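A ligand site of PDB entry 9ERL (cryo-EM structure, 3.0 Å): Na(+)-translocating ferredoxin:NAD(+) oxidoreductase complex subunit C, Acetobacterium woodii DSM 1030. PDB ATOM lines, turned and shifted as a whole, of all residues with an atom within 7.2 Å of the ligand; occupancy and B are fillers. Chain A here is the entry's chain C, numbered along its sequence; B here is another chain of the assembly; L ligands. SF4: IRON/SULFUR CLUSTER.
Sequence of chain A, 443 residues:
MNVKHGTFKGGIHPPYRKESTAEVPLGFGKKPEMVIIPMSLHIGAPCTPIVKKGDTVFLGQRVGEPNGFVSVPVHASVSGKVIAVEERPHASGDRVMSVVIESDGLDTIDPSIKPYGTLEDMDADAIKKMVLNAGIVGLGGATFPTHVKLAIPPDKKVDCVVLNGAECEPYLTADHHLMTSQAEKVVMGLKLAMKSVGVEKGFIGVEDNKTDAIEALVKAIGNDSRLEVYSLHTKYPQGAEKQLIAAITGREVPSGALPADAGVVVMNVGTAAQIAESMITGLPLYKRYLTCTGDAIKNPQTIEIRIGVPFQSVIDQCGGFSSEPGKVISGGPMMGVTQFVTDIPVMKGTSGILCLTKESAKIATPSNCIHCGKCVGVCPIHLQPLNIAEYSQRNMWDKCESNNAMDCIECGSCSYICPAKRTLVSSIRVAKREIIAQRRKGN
N of Gly 373 sits close to S2 of the ligand (3.4 Å). An iron atom (FE1) of the ligand is bound by the side-chain sulfur of Cys 372 (2.3 Å). N of Ile 370 lies close to S3 of the ligand. The backbone NH of Cys 372 sits close to a sulfur (S2) of the ligand, 3.6 Å away. An iron atom (FE2) of the ligand is bound by the side-chain sulfur (SG) of Cys 418 (2.3 Å). An iron atom (FE4) of the ligand is bound by the side-chain sulfur (SG) of Cys 369 (2.3 Å). The side-chain sulfur of Cys 375 binds an iron atom (FE3) of the ligand, 2.3 Å away.
The side-chain sulfur of Cys 369 lies close to the backbone NH of His 371, 3.7 Å away. The backbone NH of Lys 374 lies close to the side-chain sulfur of Cys 372. The side-chain sulfur (SG) of Cys 418 sits close to the backbone NH (N) of Ala 420 (3.7 Å).
CA of His 371 touches S2 of the ligand, at 3.9 Å. CD of Pro 419 touches S4 of the ligand, at 3.98 Å. Hydrophobic or aromatic side chains within 4 Å of the ligand: Pro 419. The nearest printed residue that does not touch the ligand is Leu 424 (4.02 Å).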
ATOM      1  N   SER A 367     -13.432 -28.736 -13.097  1.00  0.00           N
ATOM      2  CA  SER A 367     -14.679 -29.316 -13.579  1.00  0.00           C
ATOM      3  C   SER A 367     -14.531 -29.861 -14.990  1.00  0.00           C
ATOM      4  O   SER A 367     -13.409 -29.984 -15.505  1.00  0.00           O
ATOM      5  CB  SER A 367     -15.810 -28.282 -13.529  1.00  0.00           C
ATOM      6  OG  SER A 367     -15.897 -27.683 -12.255  1.00  0.00           O
ATOM      7  N   ASN A 368     -15.642 -30.187 -15.633  1.00  0.00           N
ATOM      8  CA  ASN A 368     -15.632 -30.713 -16.984  1.00  0.00           C
ATOM      9  C   ASN A 368     -15.292 -29.628 -17.996  1.00  0.00           C
ATOM     10  O   ASN A 368     -15.562 -28.439 -17.785  1.00  0.00           O
ATOM     11  CB  ASN A 368     -16.978 -31.336 -17.333  1.00  0.00           C
ATOM     12  CG  ASN A 368     -16.999 -32.834 -17.140  1.00  0.00           C
ATOM     13  OD1 ASN A 368     -16.051 -33.426 -16.622  1.00  0.00           O
ATOM     14  ND2 ASN A 368     -18.081 -33.472 -17.558  1.00  0.00           N
ATOM     15  N   CYS A 369     -14.701 -30.043 -19.116  1.00  0.00           N
ATOM     16  CA  CYS A 369     -14.428 -29.143 -20.226  1.00  0.00           C
ATOM     17  C   CYS A 369     -15.711 -28.843 -20.989  1.00  0.00           C
ATOM     18  O   CYS A 369     -16.517 -29.730 -21.236  1.00  0.00           O
ATOM     19  CB  CYS A 369     -13.381 -29.750 -21.166  1.00  0.00           C
ATOM     20  SG  CYS A 369     -12.747 -28.640 -22.441  1.00  0.00           S
ATOM     21  N   ILE A 370     -15.885 -27.569 -21.372  1.00  0.00           N
ATOM     22  CA  ILE A 370     -17.096 -27.119 -22.042  1.00  0.00           C
ATOM     23  C   ILE A 370     -16.830 -26.704 -23.490  1.00  0.00           C
ATOM     24  O   ILE A 370     -17.731 -26.189 -24.145  1.00  0.00           O
ATOM     25  CB  ILE A 370     -17.772 -25.975 -21.266  1.00  0.00           C
ATOM     26  CG1 ILE A 370     -16.932 -24.705 -21.336  1.00  0.00           C
ATOM     27  CG2 ILE A 370     -17.980 -26.378 -19.818  1.00  0.00           C
ATOM     28  CD1 ILE A 370     -17.614 -23.498 -20.726  1.00  0.00           C
ATOM     29  N   HIS A 371     -15.609 -26.918 -23.981  1.00  0.00           N
ATOM     30  CA  HIS A 371     -15.233 -26.678 -25.386  1.00  0.00           C
ATOM     31  C   HIS A 371     -15.453 -25.220 -25.796  1.00  0.00           C
ATOM     32  O   HIS A 371     -15.909 -24.929 -26.905  1.00  0.00           O
ATOM     33  CB  HIS A 371     -15.990 -27.614 -26.324  1.00  0.00           C
ATOM     34  CG  HIS A 371     -15.259 -28.885 -26.624  1.00  0.00           C
ATOM     35  ND1 HIS A 371     -14.605 -29.100 -27.821  1.00  0.00           N
ATOM     36  CD2 HIS A 371     -15.075 -29.999 -25.889  1.00  0.00           C
ATOM     37  CE1 HIS A 371     -14.051 -30.291 -27.801  1.00  0.00           C
ATOM     38  NE2 HIS A 371     -14.322 -30.867 -26.645  1.00  0.00           N
ATOM     39  N   CYS A 372     -15.099 -24.285 -24.912  1.00  0.00           N
ATOM     40  CA  CYS A 372     -15.245 -22.869 -25.253  1.00  0.00           C
ATOM     41  C   CYS A 372     -14.225 -22.434 -26.300  1.00  0.00           C
ATOM     42  O   CYS A 372     -14.549 -21.691 -27.223  1.00  0.00           O
ATOM     43  CB  CYS A 372     -15.137 -22.004 -23.994  1.00  0.00           C
ATOM     44  SG  CYS A 372     -13.555 -22.110 -23.144  1.00  0.00           S
ATOM     45  N   GLY A 373     -12.979 -22.891 -26.165  1.00  0.00           N
ATOM     46  CA  GLY A 373     -11.954 -22.609 -27.160  1.00  0.00           C
ATOM     47  C   GLY A 373     -11.116 -21.372 -26.917  1.00  0.00           C
ATOM     48  O   GLY A 373     -10.467 -20.905 -27.863  1.00  0.00           O
ATOM     49  N   LYS A 374     -11.104 -20.827 -25.703  1.00  0.00           N
ATOM     50  CA  LYS A 374     -10.301 -19.650 -25.423  1.00  0.00           C
ATOM     51  C   LYS A 374      -8.823 -19.980 -25.274  1.00  0.00           C
ATOM     52  O   LYS A 374      -7.960 -19.141 -25.578  1.00  0.00           O
ATOM     53  CB  LYS A 374     -10.801 -18.956 -24.151  1.00  0.00           C
ATOM     54  CG  LYS A 374     -12.284 -18.635 -24.172  1.00  0.00           C
ATOM     55  CD  LYS A 374     -12.701 -17.914 -22.903  1.00  0.00           C
ATOM     56  CE  LYS A 374     -14.209 -17.893 -22.742  1.00  0.00           C
ATOM     57  NZ  LYS A 374     -14.878 -17.082 -23.802  1.00  0.00           N
ATOM     58  N   CYS A 375      -8.503 -21.190 -24.790  1.00  0.00           N
ATOM     59  CA  CYS A 375      -7.110 -21.580 -24.622  1.00  0.00           C
ATOM     60  C   CYS A 375      -6.392 -21.681 -25.966  1.00  0.00           C
ATOM     61  O   CYS A 375      -5.185 -21.444 -26.036  1.00  0.00           O
ATOM     62  CB  CYS A 375      -7.037 -22.924 -23.885  1.00  0.00           C
ATOM     63  SG  CYS A 375      -8.137 -24.209 -24.513  1.00  0.00           S
ATOM     64  N   VAL A 376      -7.119 -22.025 -27.030  1.00  0.00           N
ATOM     65  CA  VAL A 376      -6.540 -22.001 -28.361  1.00  0.00           C
ATOM     66  C   VAL A 376      -6.260 -20.568 -28.799  1.00  0.00           C
ATOM     67  O   VAL A 376      -5.260 -20.292 -29.469  1.00  0.00           O
ATOM     68  CB  VAL A 376      -7.483 -22.719 -29.359  1.00  0.00           C
ATOM     69  CG1 VAL A 376      -6.828 -22.828 -30.719  1.00  0.00           C
ATOM     70  CG2 VAL A 376      -7.842 -24.098 -28.830  1.00  0.00           C
ATOM     71  N   PRO A 385      -4.121 -26.530 -26.285  1.00  0.00           N
ATOM     72  CA  PRO A 385      -3.844 -27.117 -24.953  1.00  0.00           C
ATOM     73  C   PRO A 385      -4.835 -28.172 -24.498  1.00  0.00           C
ATOM     74  O   PRO A 385      -4.442 -29.077 -23.752  1.00  0.00           O
ATOM     75  CB  PRO A 385      -3.871 -25.895 -24.028  1.00  0.00           C
ATOM     76  CG  PRO A 385      -3.600 -24.729 -24.920  1.00  0.00           C
ATOM     77  CD  PRO A 385      -4.249 -25.067 -26.226  1.00  0.00           C
ATOM     78  N   LEU A 386      -6.102 -28.081 -24.918  1.00  0.00           N
ATOM     79  CA  LEU A 386      -7.113 -29.012 -24.427  1.00  0.00           C
ATOM     80  C   LEU A 386      -6.815 -30.444 -24.868  1.00  0.00           C
ATOM     81  O   LEU A 386      -6.933 -31.387 -24.076  1.00  0.00           O
ATOM     82  CB  LEU A 386      -8.504 -28.580 -24.881  1.00  0.00           C
ATOM     83  CG  LEU A 386      -8.930 -28.578 -26.361  1.00  0.00           C
ATOM     84  CD1 LEU A 386     -10.423 -28.787 -26.479  1.00  0.00           C
ATOM     85  CD2 LEU A 386      -8.535 -27.290 -27.053  1.00  0.00           C
ATOM     86  N   ASN A 387      -6.403 -30.626 -26.133  1.00  0.00           N
ATOM     87  CA  ASN A 387      -6.108 -31.966 -26.624  1.00  0.00           C
ATOM     88  C   ASN A 387      -4.888 -32.565 -25.939  1.00  0.00           C
ATOM     89  O   ASN A 387      -4.893 -33.753 -25.585  1.00  0.00           O
ATOM     90  CB  ASN A 387      -5.909 -31.924 -28.144  1.00  0.00           C
ATOM     91  CG  ASN A 387      -7.179 -31.599 -28.892  1.00  0.00           C
ATOM     92  OD1 ASN A 387      -8.252 -32.095 -28.561  1.00  0.00           O
ATOM     93  ND2 ASN A 387      -7.073 -30.748 -29.901  1.00  0.00           N
ATOM     94  N   ALA A 389      -3.769 -31.829 -22.921  1.00  0.00           N
ATOM     95  CA  ALA A 389      -4.146 -32.155 -21.550  1.00  0.00           C
ATOM     96  C   ALA A 389      -4.981 -33.420 -21.474  1.00  0.00           C
ATOM     97  O   ALA A 389      -4.745 -34.276 -20.612  1.00  0.00           O
ATOM     98  CB  ALA A 389      -4.890 -30.980 -20.920  1.00  0.00           C
ATOM     99  N   GLU A 390      -5.946 -33.583 -22.385  1.00  0.00           N
ATOM    100  CA  GLU A 390      -6.790 -34.774 -22.368  1.00  0.00           C
ATOM    101  C   GLU A 390      -6.007 -36.032 -22.728  1.00  0.00           C
ATOM    102  O   GLU A 390      -6.281 -37.110 -22.193  1.00  0.00           O
ATOM    103  CB  GLU A 390      -7.979 -34.608 -23.308  1.00  0.00           C
ATOM    104  CG  GLU A 390      -8.947 -33.515 -22.904  1.00  0.00           C
ATOM    105  CD  GLU A 390      -9.879 -33.933 -21.790  1.00  0.00           C
ATOM    106  OE1 GLU A 390     -10.482 -35.019 -21.878  1.00  0.00           O
ATOM    107  OE2 GLU A 390      -9.999 -33.167 -20.804  1.00  0.00           O
ATOM    108  N   CYS A 414      -2.737 -20.124 -20.709  1.00  0.00           N
ATOM    109  CA  CYS A 414      -3.730 -21.128 -21.103  1.00  0.00           C
ATOM    110  C   CYS A 414      -4.517 -21.633 -19.896  1.00  0.00           C
ATOM    111  O   CYS A 414      -5.728 -21.865 -19.990  1.00  0.00           O
ATOM    112  CB  CYS A 414      -3.054 -22.292 -21.829  1.00  0.00           C
ATOM    113  SG  CYS A 414      -1.951 -23.298 -20.811  1.00  0.00           S
ATOM    114  N   ILE A 417      -7.097 -18.565 -18.315  1.00  0.00           N
ATOM    115  CA  ILE A 417      -8.336 -18.132 -18.944  1.00  0.00           C
ATOM    116  C   ILE A 417      -9.430 -19.203 -18.904  1.00  0.00           C
ATOM    117  O   ILE A 417     -10.559 -18.931 -19.339  1.00  0.00           O
ATOM    118  CB  ILE A 417      -8.056 -17.700 -20.404  1.00  0.00           C
ATOM    119  CG1 ILE A 417      -9.023 -16.606 -20.856  1.00  0.00           C
ATOM    120  CG2 ILE A 417      -8.079 -18.896 -21.340  1.00  0.00           C
ATOM    121  CD1 ILE A 417      -8.733 -15.259 -20.273  1.00  0.00           C
ATOM    122  N   CYS A 418      -9.140 -20.380 -18.372  1.00  0.00           N
ATOM    123  CA  CYS A 418     -10.102 -21.481 -18.411  1.00  0.00           C
ATOM    124  C   CYS A 418     -11.287 -21.205 -17.501  1.00  0.00           C
ATOM    125  O   CYS A 418     -11.093 -20.955 -16.300  1.00  0.00           O
ATOM    126  CB  CYS A 418      -9.416 -22.776 -17.991  1.00  0.00           C
ATOM    127  SG  CYS A 418     -10.318 -24.272 -18.413  1.00  0.00           S
ATOM    128  N   PRO A 419     -12.530 -21.216 -18.016  1.00  0.00           N
ATOM    129  CA  PRO A 419     -13.692 -21.067 -17.126  1.00  0.00           C
ATOM    130  C   PRO A 419     -13.891 -22.233 -16.185  1.00  0.00           C
ATOM    131  O   PRO A 419     -14.479 -22.054 -15.114  1.00  0.00           O
ATOM    132  CB  PRO A 419     -14.867 -20.919 -18.111  1.00  0.00           C
ATOM    133  CG  PRO A 419     -14.244 -20.575 -19.414  1.00  0.00           C
ATOM    134  CD  PRO A 419     -12.916 -21.239 -19.427  1.00  0.00           C
ATOM    135  N   ALA A 420     -13.446 -23.425 -16.555  1.00  0.00           N
ATOM    136  CA  ALA A 420     -13.632 -24.626 -15.743  1.00  0.00           C
ATOM    137  C   ALA A 420     -12.532 -24.818 -14.712  1.00  0.00           C
ATOM    138  O   ALA A 420     -12.591 -25.798 -13.957  1.00  0.00           O
ATOM    139  CB  ALA A 420     -13.724 -25.865 -16.640  1.00  0.00           C
ATOM    140  N   LYS A 421     -11.536 -23.930 -14.675  1.00  0.00           N
ATOM    141  CA  LYS A 421     -10.477 -23.929 -13.652  1.00  0.00           C
ATOM    142  C   LYS A 421      -9.690 -25.239 -13.657  1.00  0.00           C
ATOM    143  O   LYS A 421      -9.614 -25.937 -12.644  1.00  0.00           O
ATOM    144  CB  LYS A 421     -11.048 -23.624 -12.270  1.00  0.00           C
ATOM    145  CG  LYS A 421     -11.905 -22.368 -12.217  1.00  0.00           C
ATOM    146  CD  LYS A 421     -11.058 -21.118 -12.325  1.00  0.00           C
ATOM    147  CE  LYS A 421     -11.882 -19.857 -12.175  1.00  0.00           C
ATOM    148  NZ  LYS A 421     -12.602 -19.512 -13.434  1.00  0.00           N
ATOM    149  N   ARG A 422      -9.087 -25.554 -14.798  1.00  0.00           N
ATOM    150  CA  ARG A 422      -8.320 -26.786 -14.937  1.00  0.00           C
ATOM    151  C   ARG A 422      -6.829 -26.519 -14.755  1.00  0.00           C
ATOM    152  O   ARG A 422      -6.404 -25.405 -14.428  1.00  0.00           O
ATOM    153  CB  ARG A 422      -8.611 -27.430 -16.294  1.00  0.00           C
ATOM    154  CG  ARG A 422     -10.073 -27.433 -16.662  1.00  0.00           C
ATOM    155  CD  ARG A 422     -10.384 -28.415 -17.774  1.00  0.00           C
ATOM    156  NE  ARG A 422     -10.682 -29.745 -17.248  1.00  0.00           N
ATOM    157  CZ  ARG A 422     -10.228 -30.871 -17.770  1.00  0.00           C
ATOM    158  NH1 ARG A 422      -9.461 -30.878 -18.850  1.00  0.00           N
ATOM    159  NH2 ARG A 422     -10.549 -32.028 -17.200  1.00  0.00           N
ATOM    160  N   LEU A 424      -4.042 -27.284 -17.012  1.00  0.00           N
ATOM    161  CA  LEU A 424      -3.508 -27.705 -18.303  1.00  0.00           C
ATOM    162  C   LEU A 424      -1.979 -27.684 -18.343  1.00  0.00           C
ATOM    163  O   LEU A 424      -1.355 -28.599 -18.886  1.00  0.00           O
ATOM    164  CB  LEU A 424      -4.077 -26.807 -19.405  1.00  0.00           C
ATOM    165  CG  LEU A 424      -5.575 -26.493 -19.307  1.00  0.00           C
ATOM    166  CD1 LEU A 424      -5.980 -25.436 -20.312  1.00  0.00           C
ATOM    167  CD2 LEU A 424      -6.388 -27.749 -19.505  1.00  0.00           C
ATOM    168  N   HIS B  18     -14.520 -15.055 -14.824  1.00  0.00           N
ATOM    169  CA  HIS B  18     -15.649 -15.709 -15.461  1.00  0.00           C
ATOM    170  C   HIS B  18     -15.617 -17.216 -15.210  1.00  0.00           C
ATOM    171  O   HIS B  18     -14.561 -17.804 -14.960  1.00  0.00           O
ATOM    172  CB  HIS B  18     -15.670 -15.418 -16.956  1.00  0.00           C
ATOM    173  CG  HIS B  18     -14.520 -16.022 -17.714  1.00  0.00           C
ATOM    174  ND1 HIS B  18     -13.257 -15.475 -17.694  1.00  0.00           N
ATOM    175  CD2 HIS B  18     -14.448 -17.102 -18.516  1.00  0.00           C
ATOM    176  CE1 HIS B  18     -12.451 -16.207 -18.442  1.00  0.00           C
ATOM    177  NE2 HIS B  18     -13.155 -17.205 -18.961  1.00  0.00           N
ATOM    178  N   THR B  20     -18.503 -21.012 -15.743  1.00  0.00           N
ATOM    179  CA  THR B  20     -19.563 -21.596 -16.559  1.00  0.00           C
ATOM    180  C   THR B  20     -20.936 -21.036 -16.179  1.00  0.00           C
ATOM    181  O   THR B  20     -21.769 -20.733 -17.048  1.00  0.00           O
ATOM    182  CB  THR B  20     -19.547 -23.121 -16.408  1.00  0.00           C
ATOM    183  OG1 THR B  20     -18.249 -23.620 -16.759  1.00  0.00           O
ATOM    184  CG2 THR B  20     -20.585 -23.761 -17.324  1.00  0.00           C
ATOM    185  N   VAL B 255     -13.368 -25.125 -33.365  1.00  0.00           N
ATOM    186  CA  VAL B 255     -12.666 -24.203 -32.478  1.00  0.00           C
ATOM    187  C   VAL B 255     -11.822 -23.167 -33.224  1.00  0.00           C
ATOM    188  O   VAL B 255     -11.415 -22.176 -32.604  1.00  0.00           O
ATOM    189  CB  VAL B 255     -11.776 -24.966 -31.471  1.00  0.00           C
ATOM    190  CG1 VAL B 255     -12.623 -25.843 -30.572  1.00  0.00           C
ATOM    191  CG2 VAL B 255     -10.744 -25.797 -32.206  1.00  0.00           C
HETATM  192 FE1  SF4 L   1     -12.332 -23.925 -22.614  1.00  0.00          FE
HETATM  193 FE2  SF4 L   1     -10.750 -24.802 -20.564  1.00  0.00          FE
HETATM  194 FE3  SF4 L   1      -9.809 -24.861 -23.139  1.00  0.00          FE
HETATM  195 FE4  SF4 L   1     -11.789 -26.595 -22.361  1.00  0.00          FE
HETATM  196  S1  SF4 L   1      -9.636 -26.522 -21.581  1.00  0.00           S
HETATM  197  S2  SF4 L   1     -11.727 -25.371 -24.280  1.00  0.00           S
HETATM  198  S3  SF4 L   1     -12.950 -25.297 -20.899  1.00  0.00           S
HETATM  199  S4  SF4 L   1     -10.364 -23.015 -21.919  1.00  0.00           S
